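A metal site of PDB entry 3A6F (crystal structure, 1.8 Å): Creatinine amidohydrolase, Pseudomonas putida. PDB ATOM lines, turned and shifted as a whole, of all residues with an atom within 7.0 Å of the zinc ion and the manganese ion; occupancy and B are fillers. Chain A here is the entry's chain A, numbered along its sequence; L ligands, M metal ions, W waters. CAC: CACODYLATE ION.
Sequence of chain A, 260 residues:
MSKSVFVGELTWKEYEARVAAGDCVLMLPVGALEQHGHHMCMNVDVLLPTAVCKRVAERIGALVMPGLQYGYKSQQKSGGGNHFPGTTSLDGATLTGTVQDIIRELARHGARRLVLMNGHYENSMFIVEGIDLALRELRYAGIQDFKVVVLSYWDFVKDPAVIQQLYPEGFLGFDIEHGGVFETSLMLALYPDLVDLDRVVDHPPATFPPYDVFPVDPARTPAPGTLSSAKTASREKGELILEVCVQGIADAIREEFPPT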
ATOM      1  N   GLY A  31      24.705   6.958 -14.917  1.00  0.00           N
ATOM      2  CA  GLY A  31      23.862   7.762 -15.783  1.00  0.00           C
ATOM      3  C   GLY A  31      23.302   7.085 -17.019  1.00  0.00           C
ATOM      4  O   GLY A  31      22.834   5.947 -16.974  1.00  0.00           O
ATOM      5  N   ALA A  32      23.357   7.814 -18.136  1.00  0.00           N
ATOM      6  CA  ALA A  32      22.851   7.315 -19.399  1.00  0.00           C
ATOM      7  C   ALA A  32      23.130   8.312 -20.514  1.00  0.00           C
ATOM      8  O   ALA A  32      23.487   9.463 -20.249  1.00  0.00           O
ATOM      9  CB  ALA A  32      21.330   7.100 -19.295  1.00  0.00           C
ATOM     10  N   GLU A  34      20.979   9.710 -23.221  1.00  0.00           N
ATOM     11  CA  GLU A  34      19.563   9.739 -23.576  1.00  0.00           C
ATOM     12  C   GLU A  34      19.144  11.125 -24.078  1.00  0.00           C
ATOM     13  O   GLU A  34      19.658  12.139 -23.615  1.00  0.00           O
ATOM     14  CB  GLU A  34      18.764   9.359 -22.330  1.00  0.00           C
ATOM     15  CG  GLU A  34      17.252   9.370 -22.438  1.00  0.00           C
ATOM     16  CD  GLU A  34      16.612   9.124 -21.092  1.00  0.00           C
ATOM     17  OE1 GLU A  34      17.055   9.756 -20.112  1.00  0.00           O
ATOM     18  OE2 GLU A  34      15.670   8.314 -20.990  1.00  0.00           O
ATOM     19  N   GLN A  35      18.216  11.163 -25.038  1.00  0.00           N
ATOM     20  CA  GLN A  35      17.762  12.432 -25.573  1.00  0.00           C
ATOM     21  C   GLN A  35      17.146  13.256 -24.454  1.00  0.00           C
ATOM     22  O   GLN A  35      16.561  12.696 -23.526  1.00  0.00           O
ATOM     23  CB  GLN A  35      16.735  12.224 -26.697  1.00  0.00           C
ATOM     24  CG  GLN A  35      15.399  11.586 -26.297  1.00  0.00           C
ATOM     25  CD  GLN A  35      14.463  12.534 -25.568  1.00  0.00           C
ATOM     26  OE1 GLN A  35      14.425  13.739 -25.828  1.00  0.00           O
ATOM     27  NE2 GLN A  35      13.671  11.989 -24.638  1.00  0.00           N
ATOM     28  N   HIS A  36      17.294  14.570 -24.528  1.00  0.00           N
ATOM     29  CA  HIS A  36      16.747  15.492 -23.543  1.00  0.00           C
ATOM     30  C   HIS A  36      16.142  16.742 -24.188  1.00  0.00           C
ATOM     31  O   HIS A  36      16.449  17.870 -23.783  1.00  0.00           O
ATOM     32  CB  HIS A  36      17.812  15.909 -22.526  1.00  0.00           C
ATOM     33  CG  HIS A  36      17.960  14.960 -21.386  1.00  0.00           C
ATOM     34  ND1 HIS A  36      18.486  13.694 -21.537  1.00  0.00           N
ATOM     35  CD2 HIS A  36      17.586  15.068 -20.086  1.00  0.00           C
ATOM     36  CE1 HIS A  36      18.424  13.058 -20.370  1.00  0.00           C
ATOM     37  NE2 HIS A  36      17.880  13.866 -19.490  1.00  0.00           N
ATOM     38  N   MET A  40      18.688  20.622 -24.681  1.00  0.00           N
ATOM     39  CA  MET A  40      19.831  20.112 -23.911  1.00  0.00           C
ATOM     40  C   MET A  40      20.580  18.956 -24.556  1.00  0.00           C
ATOM     41  O   MET A  40      20.057  18.269 -25.438  1.00  0.00           O
ATOM     42  CB  MET A  40      19.379  19.661 -22.512  1.00  0.00           C
ATOM     43  CG  MET A  40      18.938  20.778 -21.598  1.00  0.00           C
ATOM     44  SD  MET A  40      18.984  20.254 -19.873  1.00  0.00           S
ATOM     45  CE  MET A  40      17.575  19.131 -19.823  1.00  0.00           C
ATOM     46  N   VAL A  44      23.222  14.448 -20.012  1.00  0.00           N
ATOM     47  CA  VAL A  44      22.726  15.061 -18.779  1.00  0.00           C
ATOM     48  C   VAL A  44      22.735  14.090 -17.580  1.00  0.00           C
ATOM     49  O   VAL A  44      23.216  14.442 -16.498  1.00  0.00           O
ATOM     50  CB  VAL A  44      21.283  15.619 -18.970  1.00  0.00           C
ATOM     51  CG1 VAL A  44      20.710  16.097 -17.633  1.00  0.00           C
ATOM     52  CG2 VAL A  44      21.301  16.772 -19.977  1.00  0.00           C
ATOM     53  N   ASP A  45      22.220  12.886 -17.768  1.00  0.00           N
ATOM     54  CA  ASP A  45      22.161  11.915 -16.671  1.00  0.00           C
ATOM     55  C   ASP A  45      23.496  11.455 -16.113  1.00  0.00           C
ATOM     56  O   ASP A  45      23.536  10.765 -15.090  1.00  0.00           O
ATOM     57  CB  ASP A  45      21.319  10.716 -17.076  1.00  0.00           C
ATOM     58  CG  ASP A  45      19.885  11.102 -17.311  1.00  0.00           C
ATOM     59  OD1 ASP A  45      19.509  12.210 -16.884  1.00  0.00           O
ATOM     60  OD2 ASP A  45      19.140  10.318 -17.916  1.00  0.00           O
ATOM     61  N   LEU A  48      24.961  15.410 -14.291  1.00  0.00           N
ATOM     62  CA  LEU A  48      24.356  15.827 -13.029  1.00  0.00           C
ATOM     63  C   LEU A  48      24.741  15.016 -11.791  1.00  0.00           C
ATOM     64  O   LEU A  48      25.205  15.583 -10.801  1.00  0.00           O
ATOM     65  CB  LEU A  48      22.823  15.890 -13.181  1.00  0.00           C
ATOM     66  CG  LEU A  48      22.310  16.908 -14.213  1.00  0.00           C
ATOM     67  CD1 LEU A  48      20.799  17.040 -14.120  1.00  0.00           C
ATOM     68  CD2 LEU A  48      22.962  18.262 -13.981  1.00  0.00           C
ATOM     69  N   TYR A  72      20.052   1.828 -18.592  1.00  0.00           N
ATOM     70  CA  TYR A  72      18.984   0.979 -19.103  1.00  0.00           C
ATOM     71  C   TYR A  72      18.068   1.706 -20.082  1.00  0.00           C
ATOM     72  O   TYR A  72      17.986   2.930 -20.093  1.00  0.00           O
ATOM     73  CB  TYR A  72      18.160   0.396 -17.953  1.00  0.00           C
ATOM     74  CG  TYR A  72      17.127  -0.570 -18.462  1.00  0.00           C
ATOM     75  CD1 TYR A  72      17.509  -1.744 -19.124  1.00  0.00           C
ATOM     76  CD2 TYR A  72      15.769  -0.283 -18.374  1.00  0.00           C
ATOM     77  CE1 TYR A  72      16.573  -2.600 -19.670  1.00  0.00           C
ATOM     78  CE2 TYR A  72      14.814  -1.130 -18.912  1.00  0.00           C
ATOM     79  CZ  TYR A  72      15.231  -2.293 -19.567  1.00  0.00           C
ATOM     80  OH  TYR A  72      14.302  -3.142 -20.116  1.00  0.00           O
ATOM     81  N   SER A  74      15.429   3.585 -22.143  1.00  0.00           N
ATOM     82  CA  SER A  74      14.560   4.703 -21.818  1.00  0.00           C
ATOM     83  C   SER A  74      13.099   4.267 -21.912  1.00  0.00           C
ATOM     84  O   SER A  74      12.695   3.624 -22.888  1.00  0.00           O
ATOM     85  CB  SER A  74      14.828   5.851 -22.801  1.00  0.00           C
ATOM     86  OG  SER A  74      14.036   6.981 -22.498  1.00  0.00           O
ATOM     87  N   SER A  78       8.957   7.900 -18.503  1.00  0.00           N
ATOM     88  CA  SER A  78       9.992   8.526 -17.693  1.00  0.00           C
ATOM     89  C   SER A  78      11.067   9.247 -18.499  1.00  0.00           C
ATOM     90  O   SER A  78      11.528  10.309 -18.098  1.00  0.00           O
ATOM     91  CB  SER A  78      10.631   7.494 -16.759  1.00  0.00           C
ATOM     92  OG  SER A  78      11.067   6.350 -17.465  1.00  0.00           O
ATOM     93  N   GLY A  79      11.456   8.675 -19.630  1.00  0.00           N
ATOM     94  CA  GLY A  79      12.485   9.288 -20.442  1.00  0.00           C
ATOM     95  C   GLY A  79      12.078   9.524 -21.892  1.00  0.00           C
ATOM     96  O   GLY A  79      12.912   9.895 -22.718  1.00  0.00           O
ATOM     97  N   GLY A 119      21.452   8.682 -11.821  1.00  0.00           N
ATOM     98  CA  GLY A 119      21.067   9.915 -12.475  1.00  0.00           C
ATOM     99  C   GLY A 119      20.035   9.664 -13.565  1.00  0.00           C
ATOM    100  O   GLY A 119      19.522  10.598 -14.187  1.00  0.00           O
ATOM    101  N   HIS A 120      19.719   8.382 -13.777  1.00  0.00           N
ATOM    102  CA  HIS A 120      18.777   7.930 -14.806  1.00  0.00           C
ATOM    103  C   HIS A 120      17.707   7.015 -14.173  1.00  0.00           C
ATOM    104  O   HIS A 120      17.981   5.864 -13.828  1.00  0.00           O
ATOM    105  CB  HIS A 120      19.577   7.201 -15.881  1.00  0.00           C
ATOM    106  CG  HIS A 120      18.766   6.650 -17.014  1.00  0.00           C
ATOM    107  ND1 HIS A 120      17.924   7.433 -17.783  1.00  0.00           N
ATOM    108  CD2 HIS A 120      18.726   5.407 -17.561  1.00  0.00           C
ATOM    109  CE1 HIS A 120      17.417   6.701 -18.761  1.00  0.00           C
ATOM    110  NE2 HIS A 120      17.885   5.464 -18.645  1.00  0.00           N
ATOM    111  N   TYR A 121      16.504   7.549 -14.022  1.00  0.00           N
ATOM    112  CA  TYR A 121      15.391   6.817 -13.407  1.00  0.00           C
ATOM    113  C   TYR A 121      15.325   5.322 -13.703  1.00  0.00           C
ATOM    114  O   TYR A 121      15.238   4.503 -12.795  1.00  0.00           O
ATOM    115  CB  TYR A 121      14.062   7.461 -13.819  1.00  0.00           C
ATOM    116  CG  TYR A 121      12.868   6.916 -13.063  1.00  0.00           C
ATOM    117  CD1 TYR A 121      12.669   7.241 -11.720  1.00  0.00           C
ATOM    118  CD2 TYR A 121      11.961   6.071 -13.687  1.00  0.00           C
ATOM    119  CE1 TYR A 121      11.573   6.734 -11.015  1.00  0.00           C
ATOM    120  CE2 TYR A 121      10.861   5.565 -12.992  1.00  0.00           C
ATOM    121  CZ  TYR A 121      10.676   5.903 -11.654  1.00  0.00           C
ATOM    122  OH  TYR A 121       9.589   5.395 -10.965  1.00  0.00           O
ATOM    123  N   GLU A 122      15.353   4.966 -14.985  1.00  0.00           N
ATOM    124  CA  GLU A 122      15.289   3.570 -15.408  1.00  0.00           C
ATOM    125  C   GLU A 122      16.384   2.631 -14.908  1.00  0.00           C
ATOM    126  O   GLU A 122      16.231   1.409 -14.991  1.00  0.00           O
ATOM    127  CB  GLU A 122      15.216   3.500 -16.939  1.00  0.00           C
ATOM    128  CG  GLU A 122      13.934   4.104 -17.536  1.00  0.00           C
ATOM    129  CD  GLU A 122      14.017   5.609 -17.771  1.00  0.00           C
ATOM    130  OE1 GLU A 122      14.717   6.298 -16.998  1.00  0.00           O
ATOM    131  OE2 GLU A 122      13.364   6.101 -18.711  1.00  0.00           O
ATOM    132  N   ASN A 123      17.485   3.170 -14.403  1.00  0.00           N
ATOM    133  CA  ASN A 123      18.583   2.330 -13.921  1.00  0.00           C
ATOM    134  C   ASN A 123      18.345   1.592 -12.617  1.00  0.00           C
ATOM    135  O   ASN A 123      18.847   0.494 -12.422  1.00  0.00           O
ATOM    136  CB  ASN A 123      19.858   3.162 -13.729  1.00  0.00           C
ATOM    137  CG  ASN A 123      20.432   3.679 -15.025  1.00  0.00           C
ATOM    138  OD1 ASN A 123      20.322   3.032 -16.074  1.00  0.00           O
ATOM    139  ND2 ASN A 123      21.090   4.825 -14.957  1.00  0.00           N
ATOM    140  N   TYR A 153      19.822  11.307  -6.697  1.00  0.00           N
ATOM    141  CA  TYR A 153      19.957  12.639  -6.132  1.00  0.00           C
ATOM    142  C   TYR A 153      18.670  13.473  -6.019  1.00  0.00           C
ATOM    143  O   TYR A 153      18.468  14.167  -5.019  1.00  0.00           O
ATOM    144  CB  TYR A 153      21.039  13.424  -6.884  1.00  0.00           C
ATOM    145  CG  TYR A 153      20.664  13.857  -8.274  1.00  0.00           C
ATOM    146  CD1 TYR A 153      20.033  15.089  -8.494  1.00  0.00           C
ATOM    147  CD2 TYR A 153      20.915  13.043  -9.376  1.00  0.00           C
ATOM    148  CE1 TYR A 153      19.660  15.494  -9.766  1.00  0.00           C
ATOM    149  CE2 TYR A 153      20.532  13.435 -10.667  1.00  0.00           C
ATOM    150  CZ  TYR A 153      19.911  14.659 -10.847  1.00  0.00           C
ATOM    151  OH  TYR A 153      19.514  15.052 -12.099  1.00  0.00           O
ATOM    152  N   TRP A 154      17.797  13.399  -7.018  1.00  0.00           N
ATOM    153  CA  TRP A 154      16.561  14.192  -6.973  1.00  0.00           C
ATOM    154  C   TRP A 154      15.632  13.897  -5.798  1.00  0.00           C
ATOM    155  O   TRP A 154      14.840  14.751  -5.408  1.00  0.00           O
ATOM    156  CB  TRP A 154      15.793  14.055  -8.304  1.00  0.00           C
ATOM    157  CG  TRP A 154      15.337  12.672  -8.633  1.00  0.00           C
ATOM    158  CD1 TRP A 154      14.268  12.006  -8.111  1.00  0.00           C
ATOM    159  CD2 TRP A 154      15.944  11.779  -9.577  1.00  0.00           C
ATOM    160  NE1 TRP A 154      14.168  10.749  -8.666  1.00  0.00           N
ATOM    161  CE2 TRP A 154      15.192  10.586  -9.564  1.00  0.00           C
ATOM    162  CE3 TRP A 154      17.060  11.871 -10.417  1.00  0.00           C
ATOM    163  CZ2 TRP A 154      15.515   9.489 -10.382  1.00  0.00           C
ATOM    164  CZ3 TRP A 154      17.386  10.773 -11.226  1.00  0.00           C
ATOM    165  CH2 TRP A 154      16.605   9.605 -11.198  1.00  0.00           C
ATOM    166  N   GLU A 177       9.237  15.138 -14.972  1.00  0.00           N
ATOM    167  CA  GLU A 177      10.499  15.850 -14.976  1.00  0.00           C
ATOM    168  C   GLU A 177      11.624  15.236 -15.816  1.00  0.00           C
ATOM    169  O   GLU A 177      12.653  14.816 -15.276  1.00  0.00           O
ATOM    170  CB  GLU A 177      11.004  16.065 -13.539  1.00  0.00           C
ATOM    171  CG  GLU A 177      10.311  17.194 -12.777  1.00  0.00           C
ATOM    172  CD  GLU A 177      10.463  18.555 -13.440  1.00  0.00           C
ATOM    173  OE1 GLU A 177      11.535  18.837 -14.002  1.00  0.00           O
ATOM    174  OE2 GLU A 177       9.515  19.360 -13.377  1.00  0.00           O
ATOM    175  N   HIS A 178      11.414  15.153 -17.125  1.00  0.00           N
ATOM    176  CA  HIS A 178      12.444  14.656 -18.017  1.00  0.00           C
ATOM    177  C   HIS A 178      12.764  15.785 -18.981  1.00  0.00           C
ATOM    178  O   HIS A 178      11.982  16.056 -19.896  1.00  0.00           O
ATOM    179  CB  HIS A 178      11.988  13.429 -18.809  1.00  0.00           C
ATOM    180  CG  HIS A 178      12.980  12.999 -19.857  1.00  0.00           C
ATOM    181  ND1 HIS A 178      14.251  12.581 -19.542  1.00  0.00           N
ATOM    182  CD2 HIS A 178      12.906  12.995 -21.210  1.00  0.00           C
ATOM    183  CE1 HIS A 178      14.919  12.335 -20.649  1.00  0.00           C
ATOM    184  NE2 HIS A 178      14.133  12.578 -21.672  1.00  0.00           N
ATOM    185  N   GLY A 179      13.900  16.433 -18.780  1.00  0.00           N
ATOM    186  CA  GLY A 179      14.274  17.549 -19.637  1.00  0.00           C
ATOM    187  C   GLY A 179      13.423  18.764 -19.294  1.00  0.00           C
ATOM    188  O   GLY A 179      13.324  19.710 -20.073  1.00  0.00           O
ATOM    189  N   GLU A 183      15.847  19.394 -14.265  1.00  0.00           N
ATOM    190  CA  GLU A 183      17.141  19.105 -14.870  1.00  0.00           C
ATOM    191  C   GLU A 183      17.720  20.306 -15.616  1.00  0.00           C
ATOM    192  O   GLU A 183      18.921  20.562 -15.558  1.00  0.00           O
ATOM    193  CB  GLU A 183      17.034  17.925 -15.833  1.00  0.00           C
ATOM    194  CG  GLU A 183      16.981  16.589 -15.146  1.00  0.00           C
ATOM    195  CD  GLU A 183      17.062  15.453 -16.134  1.00  0.00           C
ATOM    196  OE1 GLU A 183      17.753  14.478 -15.821  1.00  0.00           O
ATOM    197  OE2 GLU A 183      16.423  15.538 -17.207  1.00  0.00           O
HETATM  198 AS   CAC L   1      15.632  11.141 -15.784  1.00  0.00          AS
HETATM  199  O1  CAC L   1      15.982  11.808 -17.347  1.00  0.00           O
HETATM  200  O2  CAC L   1      16.449   9.618 -15.667  1.00  0.00           O
HETATM  201  C1  CAC L   1      16.313  12.269 -14.330  1.00  0.00           C
HETATM  202  C2  CAC L   1      13.712  10.762 -15.611  1.00  0.00           C
HETATM  203 ZN    ZN M   1      17.664  13.200 -17.515  1.00  0.00          ZN
HETATM  204 MN    MN M   2      17.111   9.489 -17.934  1.00  0.00          MN
HETATM  205  O   HOH W   1      14.867   8.887 -18.197  1.00  0.00           O
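A ring nitrogen (ND1) of His 36 is in hydrogen-bond range of the backbone carbonyl oxygen (O) of Glu 34 (2.8 Å).
The backbone NH of Gly 179 is in hydrogen-bond range of the side-chain carboxylate of Glu 183, at 3.1 Å.
The side-chain carboxylate (OE2) of Glu 34 lies within hydrogen-bond range of the side-chain hydroxyl (OG) of Ser 74.
ND1 of His 120 sits close to OE1 of Glu 122.
O of His 120 sits close to ND2 of Asn 123 (3.5 Å).
The backbone carbonyl oxygen of Tyr 72 sits at hydrogen-bond distance from a ring nitrogen (NE2) of His 120.
The nearest printed residue that does not touch the zinc ion is His 178 (4.02 Å).
Within 4 Å of the manganese ion: Glu 34, Asp 45 and His 120.
The nearest printed residue that does not touch the manganese ion is Glu 122 (4.1 Å).
The zinc ion is bound by NE2 of His 36 (2.1 Å), OE1 of Glu 183 (2.1 Å), OD1 of Asp 45 (2.2 Å) and O1 of the ligand (2.2 Å).
The zinc ion has four donor atoms within binding distance.
Slightly farther from the zinc ion lies the side-chain carboxylate (OE2) of Glu 183 (2.7 Å).
The manganese ion is bound by the side-chain carboxylate of Asp 45 (2.2 Å), the side-chain carboxylate of Glu 34 (2.2 Å), a ring nitrogen (ND1) of His 120 (2.2 Å), water W1 (2.3 Å), an oxygen (O2) of the ligand (2.4 Å) and an oxygen (O1) of the ligand (2.6 Å).
The manganese ion has six donor atoms within binding distance.
Water W1 bridges the side-chain carboxylate (OE1) of Glu 122 (2.9 Å) and the side-chain carboxylate (OE2) of Glu 34 (3.0 Å).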
